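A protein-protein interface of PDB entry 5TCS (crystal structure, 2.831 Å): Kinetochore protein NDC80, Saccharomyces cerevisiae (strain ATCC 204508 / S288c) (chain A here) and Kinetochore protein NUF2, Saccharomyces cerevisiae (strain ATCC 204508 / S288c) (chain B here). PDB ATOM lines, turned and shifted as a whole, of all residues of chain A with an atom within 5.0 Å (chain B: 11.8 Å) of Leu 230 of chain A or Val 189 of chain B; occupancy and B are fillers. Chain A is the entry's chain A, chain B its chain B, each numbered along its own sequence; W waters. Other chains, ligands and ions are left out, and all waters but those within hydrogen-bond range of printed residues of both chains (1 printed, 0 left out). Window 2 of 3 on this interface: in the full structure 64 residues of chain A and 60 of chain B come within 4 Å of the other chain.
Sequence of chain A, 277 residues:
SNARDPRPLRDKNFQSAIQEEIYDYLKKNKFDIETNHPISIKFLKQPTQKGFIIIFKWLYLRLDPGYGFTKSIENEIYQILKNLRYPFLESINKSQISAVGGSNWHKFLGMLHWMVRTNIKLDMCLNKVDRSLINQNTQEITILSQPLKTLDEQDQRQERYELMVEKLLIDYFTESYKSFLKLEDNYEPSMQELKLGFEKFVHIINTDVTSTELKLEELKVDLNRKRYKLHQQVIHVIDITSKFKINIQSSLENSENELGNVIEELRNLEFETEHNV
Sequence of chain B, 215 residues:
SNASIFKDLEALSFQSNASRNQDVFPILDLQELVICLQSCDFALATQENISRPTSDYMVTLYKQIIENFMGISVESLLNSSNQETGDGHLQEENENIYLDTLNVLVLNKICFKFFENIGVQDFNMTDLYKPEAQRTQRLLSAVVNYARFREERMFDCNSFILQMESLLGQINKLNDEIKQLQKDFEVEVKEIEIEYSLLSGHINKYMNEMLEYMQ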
ATOM      1  N   LYS A 226      27.743  34.553   7.503  1.00  0.00           N
ATOM      2  CA  LYS A 226      27.521  33.124   7.314  1.00  0.00           C
ATOM      3  C   LYS A 226      27.535  32.763   5.833  1.00  0.00           C
ATOM      4  O   LYS A 226      28.226  31.824   5.419  1.00  0.00           O
ATOM      5  CB  LYS A 226      26.198  32.707   7.959  1.00  0.00           C
ATOM      6  CG  LYS A 226      26.096  33.020   9.448  1.00  0.00           C
ATOM      7  CD  LYS A 226      25.420  31.882  10.217  1.00  0.00           C
ATOM      8  CE  LYS A 226      24.348  32.371  11.184  1.00  0.00           C
ATOM      9  NZ  LYS A 226      24.865  32.574  12.566  1.00  0.00           N
ATOM     10  N   ARG A 227      26.777  33.504   5.022  1.00  0.00           N
ATOM     11  CA  ARG A 227      26.740  33.270   3.583  1.00  0.00           C
ATOM     12  C   ARG A 227      28.145  33.101   3.018  1.00  0.00           C
ATOM     13  O   ARG A 227      28.469  32.071   2.416  1.00  0.00           O
ATOM     14  CB  ARG A 227      26.015  34.427   2.898  1.00  0.00           C
ATOM     15  CG  ARG A 227      25.942  34.321   1.382  1.00  0.00           C
ATOM     16  CD  ARG A 227      24.534  34.607   0.901  1.00  0.00           C
ATOM     17  NE  ARG A 227      24.006  35.838   1.491  1.00  0.00           N
ATOM     18  CZ  ARG A 227      22.758  36.005   1.922  1.00  0.00           C
ATOM     19  NH1 ARG A 227      21.876  35.016   1.851  1.00  0.00           N
ATOM     20  NH2 ARG A 227      22.391  37.169   2.440  1.00  0.00           N
ATOM     21  N   TYR A 228      28.994  34.114   3.200  1.00  0.00           N
ATOM     22  CA  TYR A 228      30.390  33.992   2.800  1.00  0.00           C
ATOM     23  C   TYR A 228      30.980  32.691   3.327  1.00  0.00           C
ATOM     24  O   TYR A 228      31.419  31.830   2.555  1.00  0.00           O
ATOM     25  CB  TYR A 228      31.187  35.198   3.308  1.00  0.00           C
ATOM     26  CG  TYR A 228      32.662  35.129   2.985  1.00  0.00           C
ATOM     27  CD1 TYR A 228      33.143  35.560   1.754  1.00  0.00           C
ATOM     28  CD2 TYR A 228      33.574  34.631   3.906  1.00  0.00           C
ATOM     29  CE1 TYR A 228      34.490  35.496   1.450  1.00  0.00           C
ATOM     30  CE2 TYR A 228      34.923  34.564   3.613  1.00  0.00           C
ATOM     31  CZ  TYR A 228      35.376  34.998   2.382  1.00  0.00           C
ATOM     32  OH  TYR A 228      36.718  34.935   2.082  1.00  0.00           O
ATOM     33  N   LYS A 229      30.964  32.522   4.653  1.00  0.00           N
ATOM     34  CA  LYS A 229      31.477  31.302   5.266  1.00  0.00           C
ATOM     35  C   LYS A 229      30.976  30.066   4.533  1.00  0.00           C
ATOM     36  O   LYS A 229      31.731  29.113   4.310  1.00  0.00           O
ATOM     37  CB  LYS A 229      31.060  31.246   6.736  1.00  0.00           C
ATOM     38  CG  LYS A 229      32.083  30.616   7.668  1.00  0.00           C
ATOM     39  CD  LYS A 229      33.208  31.588   8.000  1.00  0.00           C
ATOM     40  CE  LYS A 229      33.978  31.156   9.239  1.00  0.00           C
ATOM     41  NZ  LYS A 229      33.143  31.233  10.476  1.00  0.00           N
ATOM     42  N   LEU A 230      29.701  30.069   4.140  1.00  0.00           N
ATOM     43  CA  LEU A 230      29.136  28.915   3.452  1.00  0.00           C
ATOM     44  C   LEU A 230      29.707  28.783   2.049  1.00  0.00           C
ATOM     45  O   LEU A 230      30.190  27.712   1.664  1.00  0.00           O
ATOM     46  CB  LEU A 230      27.612  29.027   3.399  1.00  0.00           C
ATOM     47  CG  LEU A 230      26.890  27.866   2.711  1.00  0.00           C
ATOM     48  CD1 LEU A 230      27.168  26.552   3.428  1.00  0.00           C
ATOM     49  CD2 LEU A 230      25.397  28.134   2.643  1.00  0.00           C
ATOM     50  N   HIS A 231      29.660  29.860   1.264  1.00  0.00           N
ATOM     51  CA  HIS A 231      30.117  29.769  -0.117  1.00  0.00           C
ATOM     52  C   HIS A 231      31.546  29.248  -0.176  1.00  0.00           C
ATOM     53  O   HIS A 231      31.857  28.341  -0.960  1.00  0.00           O
ATOM     54  CB  HIS A 231      29.993  31.130  -0.802  1.00  0.00           C
ATOM     55  CG  HIS A 231      28.588  31.479  -1.184  1.00  0.00           C
ATOM     56  ND1 HIS A 231      28.286  32.450  -2.115  1.00  0.00           N
ATOM     57  CD2 HIS A 231      27.400  30.984  -0.760  1.00  0.00           C
ATOM     58  CE1 HIS A 231      26.975  32.537  -2.248  1.00  0.00           C
ATOM     59  NE2 HIS A 231      26.413  31.659  -1.437  1.00  0.00           N
ATOM     60  N   GLN A 232      32.424  29.788   0.672  1.00  0.00           N
ATOM     61  CA  GLN A 232      33.779  29.259   0.779  1.00  0.00           C
ATOM     62  C   GLN A 232      33.753  27.738   0.865  1.00  0.00           C
ATOM     63  O   GLN A 232      34.331  27.045   0.020  1.00  0.00           O
ATOM     64  CB  GLN A 232      34.480  29.864   1.999  1.00  0.00           C
ATOM     65  CG  GLN A 232      34.620  31.381   1.953  1.00  0.00           C
ATOM     66  CD  GLN A 232      35.432  31.861   0.764  1.00  0.00           C
ATOM     67  OE1 GLN A 232      34.926  32.576  -0.101  1.00  0.00           O
ATOM     68  NE2 GLN A 232      36.701  31.477   0.721  1.00  0.00           N
ATOM     69  N   GLN A 233      33.057  27.201   1.872  1.00  0.00           N
ATOM     70  CA  GLN A 233      32.903  25.756   2.000  1.00  0.00           C
ATOM     71  C   GLN A 233      32.575  25.121   0.654  1.00  0.00           C
ATOM     72  O   GLN A 233      33.291  24.232   0.181  1.00  0.00           O
ATOM     73  CB  GLN A 233      31.814  25.421   3.025  1.00  0.00           C
ATOM     74  CG  GLN A 233      32.202  25.667   4.471  1.00  0.00           C
ATOM     75  CD  GLN A 233      31.105  25.259   5.436  1.00  0.00           C
ATOM     76  OE1 GLN A 233      29.989  25.777   5.381  1.00  0.00           O
ATOM     77  NE2 GLN A 233      31.414  24.317   6.319  1.00  0.00           N
ATOM     78  N   VAL A 234      31.498  25.587   0.013  1.00  0.00           N
ATOM     79  CA  VAL A 234      31.118  25.053  -1.294  1.00  0.00           C
ATOM     80  C   VAL A 234      32.326  25.069  -2.223  1.00  0.00           C
ATOM     81  O   VAL A 234      32.756  24.032  -2.736  1.00  0.00           O
ATOM     82  CB  VAL A 234      29.939  25.848  -1.880  1.00  0.00           C
ATOM     83  CG1 VAL A 234      29.866  25.700  -3.399  1.00  0.00           C
ATOM     84  CG2 VAL A 234      28.640  25.375  -1.250  1.00  0.00           C
ATOM     85  N   GLN B 180      11.590  37.303   7.383  1.00  0.00           N
ATOM     86  CA  GLN B 180      11.813  37.118   5.955  1.00  0.00           C
ATOM     87  C   GLN B 180      13.284  36.852   5.664  1.00  0.00           C
ATOM     88  O   GLN B 180      13.622  35.931   4.911  1.00  0.00           O
ATOM     89  CB  GLN B 180      11.325  38.346   5.186  1.00  0.00           C
ATOM     90  CG  GLN B 180      11.041  38.077   3.718  1.00  0.00           C
ATOM     91  CD  GLN B 180       9.961  37.028   3.522  1.00  0.00           C
ATOM     92  OE1 GLN B 180       8.877  37.122   4.098  1.00  0.00           O
ATOM     93  NE2 GLN B 180      10.261  36.013   2.718  1.00  0.00           N
ATOM     94  N   LEU B 181      14.176  37.654   6.249  1.00  0.00           N
ATOM     95  CA  LEU B 181      15.607  37.443   6.057  1.00  0.00           C
ATOM     96  C   LEU B 181      16.014  36.028   6.453  1.00  0.00           C
ATOM     97  O   LEU B 181      16.560  35.270   5.641  1.00  0.00           O
ATOM     98  CB  LEU B 181      16.395  38.475   6.864  1.00  0.00           C
ATOM     99  CG  LEU B 181      16.469  39.872   6.250  1.00  0.00           C
ATOM    100  CD1 LEU B 181      16.651  40.918   7.332  1.00  0.00           C
ATOM    101  CD2 LEU B 181      17.603  39.946   5.243  1.00  0.00           C
ATOM    102  N   GLN B 182      15.757  35.655   7.709  1.00  0.00           N
ATOM    103  CA  GLN B 182      16.216  34.349   8.174  1.00  0.00           C
ATOM    104  C   GLN B 182      15.546  33.214   7.409  1.00  0.00           C
ATOM    105  O   GLN B 182      16.164  32.165   7.190  1.00  0.00           O
ATOM    106  CB  GLN B 182      15.990  34.212   9.680  1.00  0.00           C
ATOM    107  CG  GLN B 182      14.560  34.447  10.159  1.00  0.00           C
ATOM    108  CD  GLN B 182      14.466  34.765  11.651  1.00  0.00           C
ATOM    109  OE1 GLN B 182      13.410  35.170  12.132  1.00  0.00           O
ATOM    110  NE2 GLN B 182      15.562  34.583  12.386  1.00  0.00           N
ATOM    111  N   LYS B 183      14.298  33.408   6.973  1.00  0.00           N
ATOM    112  CA  LYS B 183      13.644  32.410   6.129  1.00  0.00           C
ATOM    113  C   LYS B 183      14.395  32.237   4.813  1.00  0.00           C
ATOM    114  O   LYS B 183      14.728  31.114   4.416  1.00  0.00           O
ATOM    115  CB  LYS B 183      12.193  32.821   5.877  1.00  0.00           C
ATOM    116  CG  LYS B 183      11.326  31.752   5.224  1.00  0.00           C
ATOM    117  CD  LYS B 183       9.850  32.033   5.480  1.00  0.00           C
ATOM    118  CE  LYS B 183       8.941  31.158   4.630  1.00  0.00           C
ATOM    119  NZ  LYS B 183       7.508  31.538   4.790  1.00  0.00           N
ATOM    120  N   ASP B 184      14.671  33.346   4.124  1.00  0.00           N
ATOM    121  CA  ASP B 184      15.423  33.300   2.875  1.00  0.00           C
ATOM    122  C   ASP B 184      16.745  32.562   3.055  1.00  0.00           C
ATOM    123  O   ASP B 184      17.042  31.592   2.344  1.00  0.00           O
ATOM    124  CB  ASP B 184      15.668  34.725   2.372  1.00  0.00           C
ATOM    125  CG  ASP B 184      14.400  35.401   1.885  1.00  0.00           C
ATOM    126  OD1 ASP B 184      13.306  34.829   2.075  1.00  0.00           O
ATOM    127  OD2 ASP B 184      14.496  36.510   1.317  1.00  0.00           O
ATOM    128  N   PHE B 185      17.562  33.019   4.009  1.00  0.00           N
ATOM    129  CA  PHE B 185      18.859  32.386   4.214  1.00  0.00           C
ATOM    130  C   PHE B 185      18.709  30.898   4.501  1.00  0.00           C
ATOM    131  O   PHE B 185      19.455  30.072   3.955  1.00  0.00           O
ATOM    132  CB  PHE B 185      19.609  33.074   5.353  1.00  0.00           C
ATOM    133  CG  PHE B 185      20.974  32.505   5.601  1.00  0.00           C
ATOM    134  CD1 PHE B 185      21.973  32.638   4.652  1.00  0.00           C
ATOM    135  CD2 PHE B 185      21.258  31.836   6.779  1.00  0.00           C
ATOM    136  CE1 PHE B 185      23.231  32.116   4.874  1.00  0.00           C
ATOM    137  CE2 PHE B 185      22.515  31.312   7.006  1.00  0.00           C
ATOM    138  CZ  PHE B 185      23.502  31.452   6.053  1.00  0.00           C
ATOM    139  N   GLU B 186      17.749  30.533   5.354  1.00  0.00           N
ATOM    140  CA  GLU B 186      17.517  29.120   5.636  1.00  0.00           C
ATOM    141  C   GLU B 186      17.200  28.351   4.362  1.00  0.00           C
ATOM    142  O   GLU B 186      17.635  27.206   4.194  1.00  0.00           O
ATOM    143  CB  GLU B 186      16.386  28.964   6.650  1.00  0.00           C
ATOM    144  CG  GLU B 186      16.813  28.299   7.944  1.00  0.00           C
ATOM    145  CD  GLU B 186      15.848  28.571   9.079  1.00  0.00           C
ATOM    146  OE1 GLU B 186      14.644  28.284   8.917  1.00  0.00           O
ATOM    147  OE2 GLU B 186      16.293  29.087  10.128  1.00  0.00           O
ATOM    148  N   VAL B 187      16.438  28.960   3.452  1.00  0.00           N
ATOM    149  CA  VAL B 187      16.160  28.318   2.169  1.00  0.00           C
ATOM    150  C   VAL B 187      17.456  28.084   1.408  1.00  0.00           C
ATOM    151  O   VAL B 187      17.713  26.981   0.909  1.00  0.00           O
ATOM    152  CB  VAL B 187      15.162  29.162   1.353  1.00  0.00           C
ATOM    153  CG1 VAL B 187      15.255  28.844  -0.141  1.00  0.00           C
ATOM    154  CG2 VAL B 187      13.748  28.914   1.852  1.00  0.00           C
ATOM    155  N   GLU B 188      18.295  29.118   1.302  1.00  0.00           N
ATOM    156  CA  GLU B 188      19.580  28.955   0.626  1.00  0.00           C
ATOM    157  C   GLU B 188      20.353  27.771   1.198  1.00  0.00           C
ATOM    158  O   GLU B 188      20.772  26.867   0.461  1.00  0.00           O
ATOM    159  CB  GLU B 188      20.399  30.240   0.746  1.00  0.00           C
ATOM    160  CG  GLU B 188      19.787  31.432   0.035  1.00  0.00           C
ATOM    161  CD  GLU B 188      20.579  32.704   0.250  1.00  0.00           C
ATOM    162  OE1 GLU B 188      21.825  32.645   0.189  1.00  0.00           O
ATOM    163  OE2 GLU B 188      19.957  33.760   0.491  1.00  0.00           O
ATOM    164  N   VAL B 189      20.549  27.761   2.520  1.00  0.00           N
ATOM    165  CA  VAL B 189      21.241  26.648   3.168  1.00  0.00           C
ATOM    166  C   VAL B 189      20.582  25.326   2.803  1.00  0.00           C
ATOM    167  O   VAL B 189      21.259  24.307   2.615  1.00  0.00           O
ATOM    168  CB  VAL B 189      21.276  26.864   4.694  1.00  0.00           C
ATOM    169  CG1 VAL B 189      21.685  25.584   5.424  1.00  0.00           C
ATOM    170  CG2 VAL B 189      22.228  27.995   5.038  1.00  0.00           C
ATOM    171  N   LYS B 190      19.252  25.317   2.703  1.00  0.00           N
ATOM    172  CA  LYS B 190      18.546  24.088   2.357  1.00  0.00           C
ATOM    173  C   LYS B 190      18.949  23.602   0.972  1.00  0.00           C
ATOM    174  O   LYS B 190      19.369  22.451   0.800  1.00  0.00           O
ATOM    175  CB  LYS B 190      17.036  24.316   2.428  1.00  0.00           C
ATOM    176  CG  LYS B 190      16.215  23.039   2.401  1.00  0.00           C
ATOM    177  CD  LYS B 190      14.730  23.336   2.271  1.00  0.00           C
ATOM    178  CE  LYS B 190      13.900  22.065   2.348  1.00  0.00           C
ATOM    179  NZ  LYS B 190      12.532  22.326   2.880  1.00  0.00           N
ATOM    180  N   GLU B 191      18.831  24.471  -0.033  1.00  0.00           N
ATOM    181  CA  GLU B 191      19.150  24.076  -1.402  1.00  0.00           C
ATOM    182  C   GLU B 191      20.595  23.603  -1.508  1.00  0.00           C
ATOM    183  O   GLU B 191      20.876  22.538  -2.078  1.00  0.00           O
ATOM    184  CB  GLU B 191      18.888  25.243  -2.355  1.00  0.00           C
ATOM    185  CG  GLU B 191      17.525  25.895  -2.171  1.00  0.00           C
ATOM    186  CD  GLU B 191      17.084  26.688  -3.383  1.00  0.00           C
ATOM    187  OE1 GLU B 191      17.958  27.117  -4.164  1.00  0.00           O
ATOM    188  OE2 GLU B 191      15.860  26.881  -3.556  1.00  0.00           O
ATOM    189  N   ILE B 192      21.530  24.380  -0.954  1.00  0.00           N
ATOM    190  CA  ILE B 192      22.937  23.994  -1.021  1.00  0.00           C
ATOM    191  C   ILE B 192      23.146  22.636  -0.368  1.00  0.00           C
ATOM    192  O   ILE B 192      23.781  21.745  -0.941  1.00  0.00           O
ATOM    193  CB  ILE B 192      23.824  25.075  -0.379  1.00  0.00           C
ATOM    194  CG1 ILE B 192      23.850  26.317  -1.274  1.00  0.00           C
ATOM    195  CG2 ILE B 192      25.245  24.537  -0.148  1.00  0.00           C
ATOM    196  CD1 ILE B 192      24.635  27.485  -0.708  1.00  0.00           C
ATOM    197  N   GLU B 193      22.628  22.458   0.850  1.00  0.00           N
ATOM    198  CA  GLU B 193      22.776  21.170   1.524  1.00  0.00           C
ATOM    199  C   GLU B 193      22.218  20.038   0.669  1.00  0.00           C
ATOM    200  O   GLU B 193      22.774  18.934   0.647  1.00  0.00           O
ATOM    201  CB  GLU B 193      22.084  21.207   2.889  1.00  0.00           C
ATOM    202  CG  GLU B 193      22.844  21.976   3.965  1.00  0.00           C
ATOM    203  CD  GLU B 193      24.067  21.233   4.478  1.00  0.00           C
ATOM    204  OE1 GLU B 193      24.614  20.388   3.737  1.00  0.00           O
ATOM    205  OE2 GLU B 193      24.478  21.487   5.630  1.00  0.00           O
ATOM    206  N   ILE B 194      21.126  20.299  -0.051  1.00  0.00           N
ATOM    207  CA  ILE B 194      20.549  19.284  -0.929  1.00  0.00           C
ATOM    208  C   ILE B 194      21.548  18.899  -2.016  1.00  0.00           C
ATOM    209  O   ILE B 194      21.928  17.728  -2.156  1.00  0.00           O
ATOM    210  CB  ILE B 194      19.220  19.787  -1.523  1.00  0.00           C
ATOM    211  CG1 ILE B 194      18.075  19.491  -0.550  1.00  0.00           C
ATOM    212  CG2 ILE B 194      18.933  19.156  -2.891  1.00  0.00           C
ATOM    213  CD1 ILE B 194      16.784  20.213  -0.872  1.00  0.00           C
ATOM    214  N   GLU B 195      21.997  19.882  -2.800  1.00  0.00           N
ATOM    215  CA  GLU B 195      22.915  19.567  -3.890  1.00  0.00           C
ATOM    216  C   GLU B 195      24.170  18.884  -3.366  1.00  0.00           C
ATOM    217  O   GLU B 195      24.617  17.875  -3.921  1.00  0.00           O
ATOM    218  CB  GLU B 195      23.277  20.829  -4.670  1.00  0.00           C
ATOM    219  CG  GLU B 195      22.333  21.140  -5.819  1.00  0.00           C
ATOM    220  CD  GLU B 195      22.255  20.024  -6.847  1.00  0.00           C
ATOM    221  OE1 GLU B 195      23.235  19.262  -6.971  1.00  0.00           O
ATOM    222  OE2 GLU B 195      21.213  19.910  -7.531  1.00  0.00           O
ATOM    223  N   TYR B 196      24.758  19.420  -2.295  1.00  0.00           N
ATOM    224  CA  TYR B 196      25.933  18.780  -1.719  1.00  0.00           C
ATOM    225  C   TYR B 196      25.646  17.333  -1.363  1.00  0.00           C
ATOM    226  O   TYR B 196      26.491  16.460  -1.573  1.00  0.00           O
ATOM    227  CB  TYR B 196      26.417  19.519  -0.472  1.00  0.00           C
ATOM    228  CG  TYR B 196      27.474  18.722   0.263  1.00  0.00           C
ATOM    229  CD1 TYR B 196      28.810  18.797  -0.108  1.00  0.00           C
ATOM    230  CD2 TYR B 196      27.131  17.865   1.302  1.00  0.00           C
ATOM    231  CE1 TYR B 196      29.777  18.058   0.546  1.00  0.00           C
ATOM    232  CE2 TYR B 196      28.090  17.120   1.960  1.00  0.00           C
ATOM    233  CZ  TYR B 196      29.412  17.222   1.578  1.00  0.00           C
ATOM    234  OH  TYR B 196      30.371  16.484   2.234  1.00  0.00           O
ATOM    235  N   SER B 197      24.473  17.057  -0.788  1.00  0.00           N
ATOM    236  CA  SER B 197      24.140  15.675  -0.462  1.00  0.00           C
ATOM    237  C   SER B 197      24.124  14.809  -1.715  1.00  0.00           C
ATOM    238  O   SER B 197      24.650  13.687  -1.712  1.00  0.00           O
ATOM    239  CB  SER B 197      22.795  15.604   0.258  1.00  0.00           C
ATOM    240  OG  SER B 197      21.739  15.966  -0.610  1.00  0.00           O
ATOM    241  N   LEU B 198      23.526  15.311  -2.799  1.00  0.00           N
ATOM    242  CA  LEU B 198      23.543  14.560  -4.052  1.00  0.00           C
ATOM    243  C   LEU B 198      24.972  14.312  -4.528  1.00  0.00           C
ATOM    244  O   LEU B 198      25.285  13.229  -5.038  1.00  0.00           O
ATOM    245  CB  LEU B 198      22.745  15.305  -5.122  1.00  0.00           C
ATOM    246  CG  LEU B 198      21.232  15.423  -4.907  1.00  0.00           C
ATOM    247  CD1 LEU B 198      20.577  16.050  -6.131  1.00  0.00           C
ATOM    248  CD2 LEU B 198      20.597  14.071  -4.601  1.00  0.00           C
HETATM  249  O   HOH W   1      23.719  31.587  -1.817  1.00  0.00           O
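Hydrophobic or aromatic side chains of chain B within 4 Å of the printed part of chain A: Phe 185, Val 189 and Ile 192.
Among the printed residues, 6 pairs touch across the chains.
OE2 of Glu 188 of chain B lies within salt-bridge range of NH1 of Arg 227 of chain A (2.7 Å).
Among the printed residues, pairs that only touch across the chains: Lys 226 of chain A with Phe 185 of chain B, Arg 227 of chain A with Phe 185 of chain B, Leu 230 of chain A with Val 189 of chain B, Leu 230 of chain A with Ile 192 of chain B and Val 234 of chain A with Ile 192 of chain B.
Water W1 bridges a ring nitrogen (NE2) of His 231 of chain A (2.7 Å) and the side-chain carboxylate of Glu 188 of chain B (3.0 Å).
Printed residues of chain B within 4 Å of Lys 226 of chain A: Phe 185.
No residue of chain B comes within 4 Å of Lys 229 of chain A.
Leu 230 of chain A touches two residues of chain B.
Val 234 of chain A touches just one residue of chain B: Ile 192 (3.7 Å).
Gln 180 of chain B touches none of the printed residues of chain A.
Lys 183 of chain B touches none of the printed residues of chain A.
Printed residues of chain A within 4 Å of Phe 185 of chain B: Lys 226 (3.5 Å) and Arg 227 (3.7 Å).
Val 189 of chain B touches one residue of chain A.
The nearest printed residue of chain A that does not touch Ile 192 of chain B is His 231 of chain A (4.5 Å).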
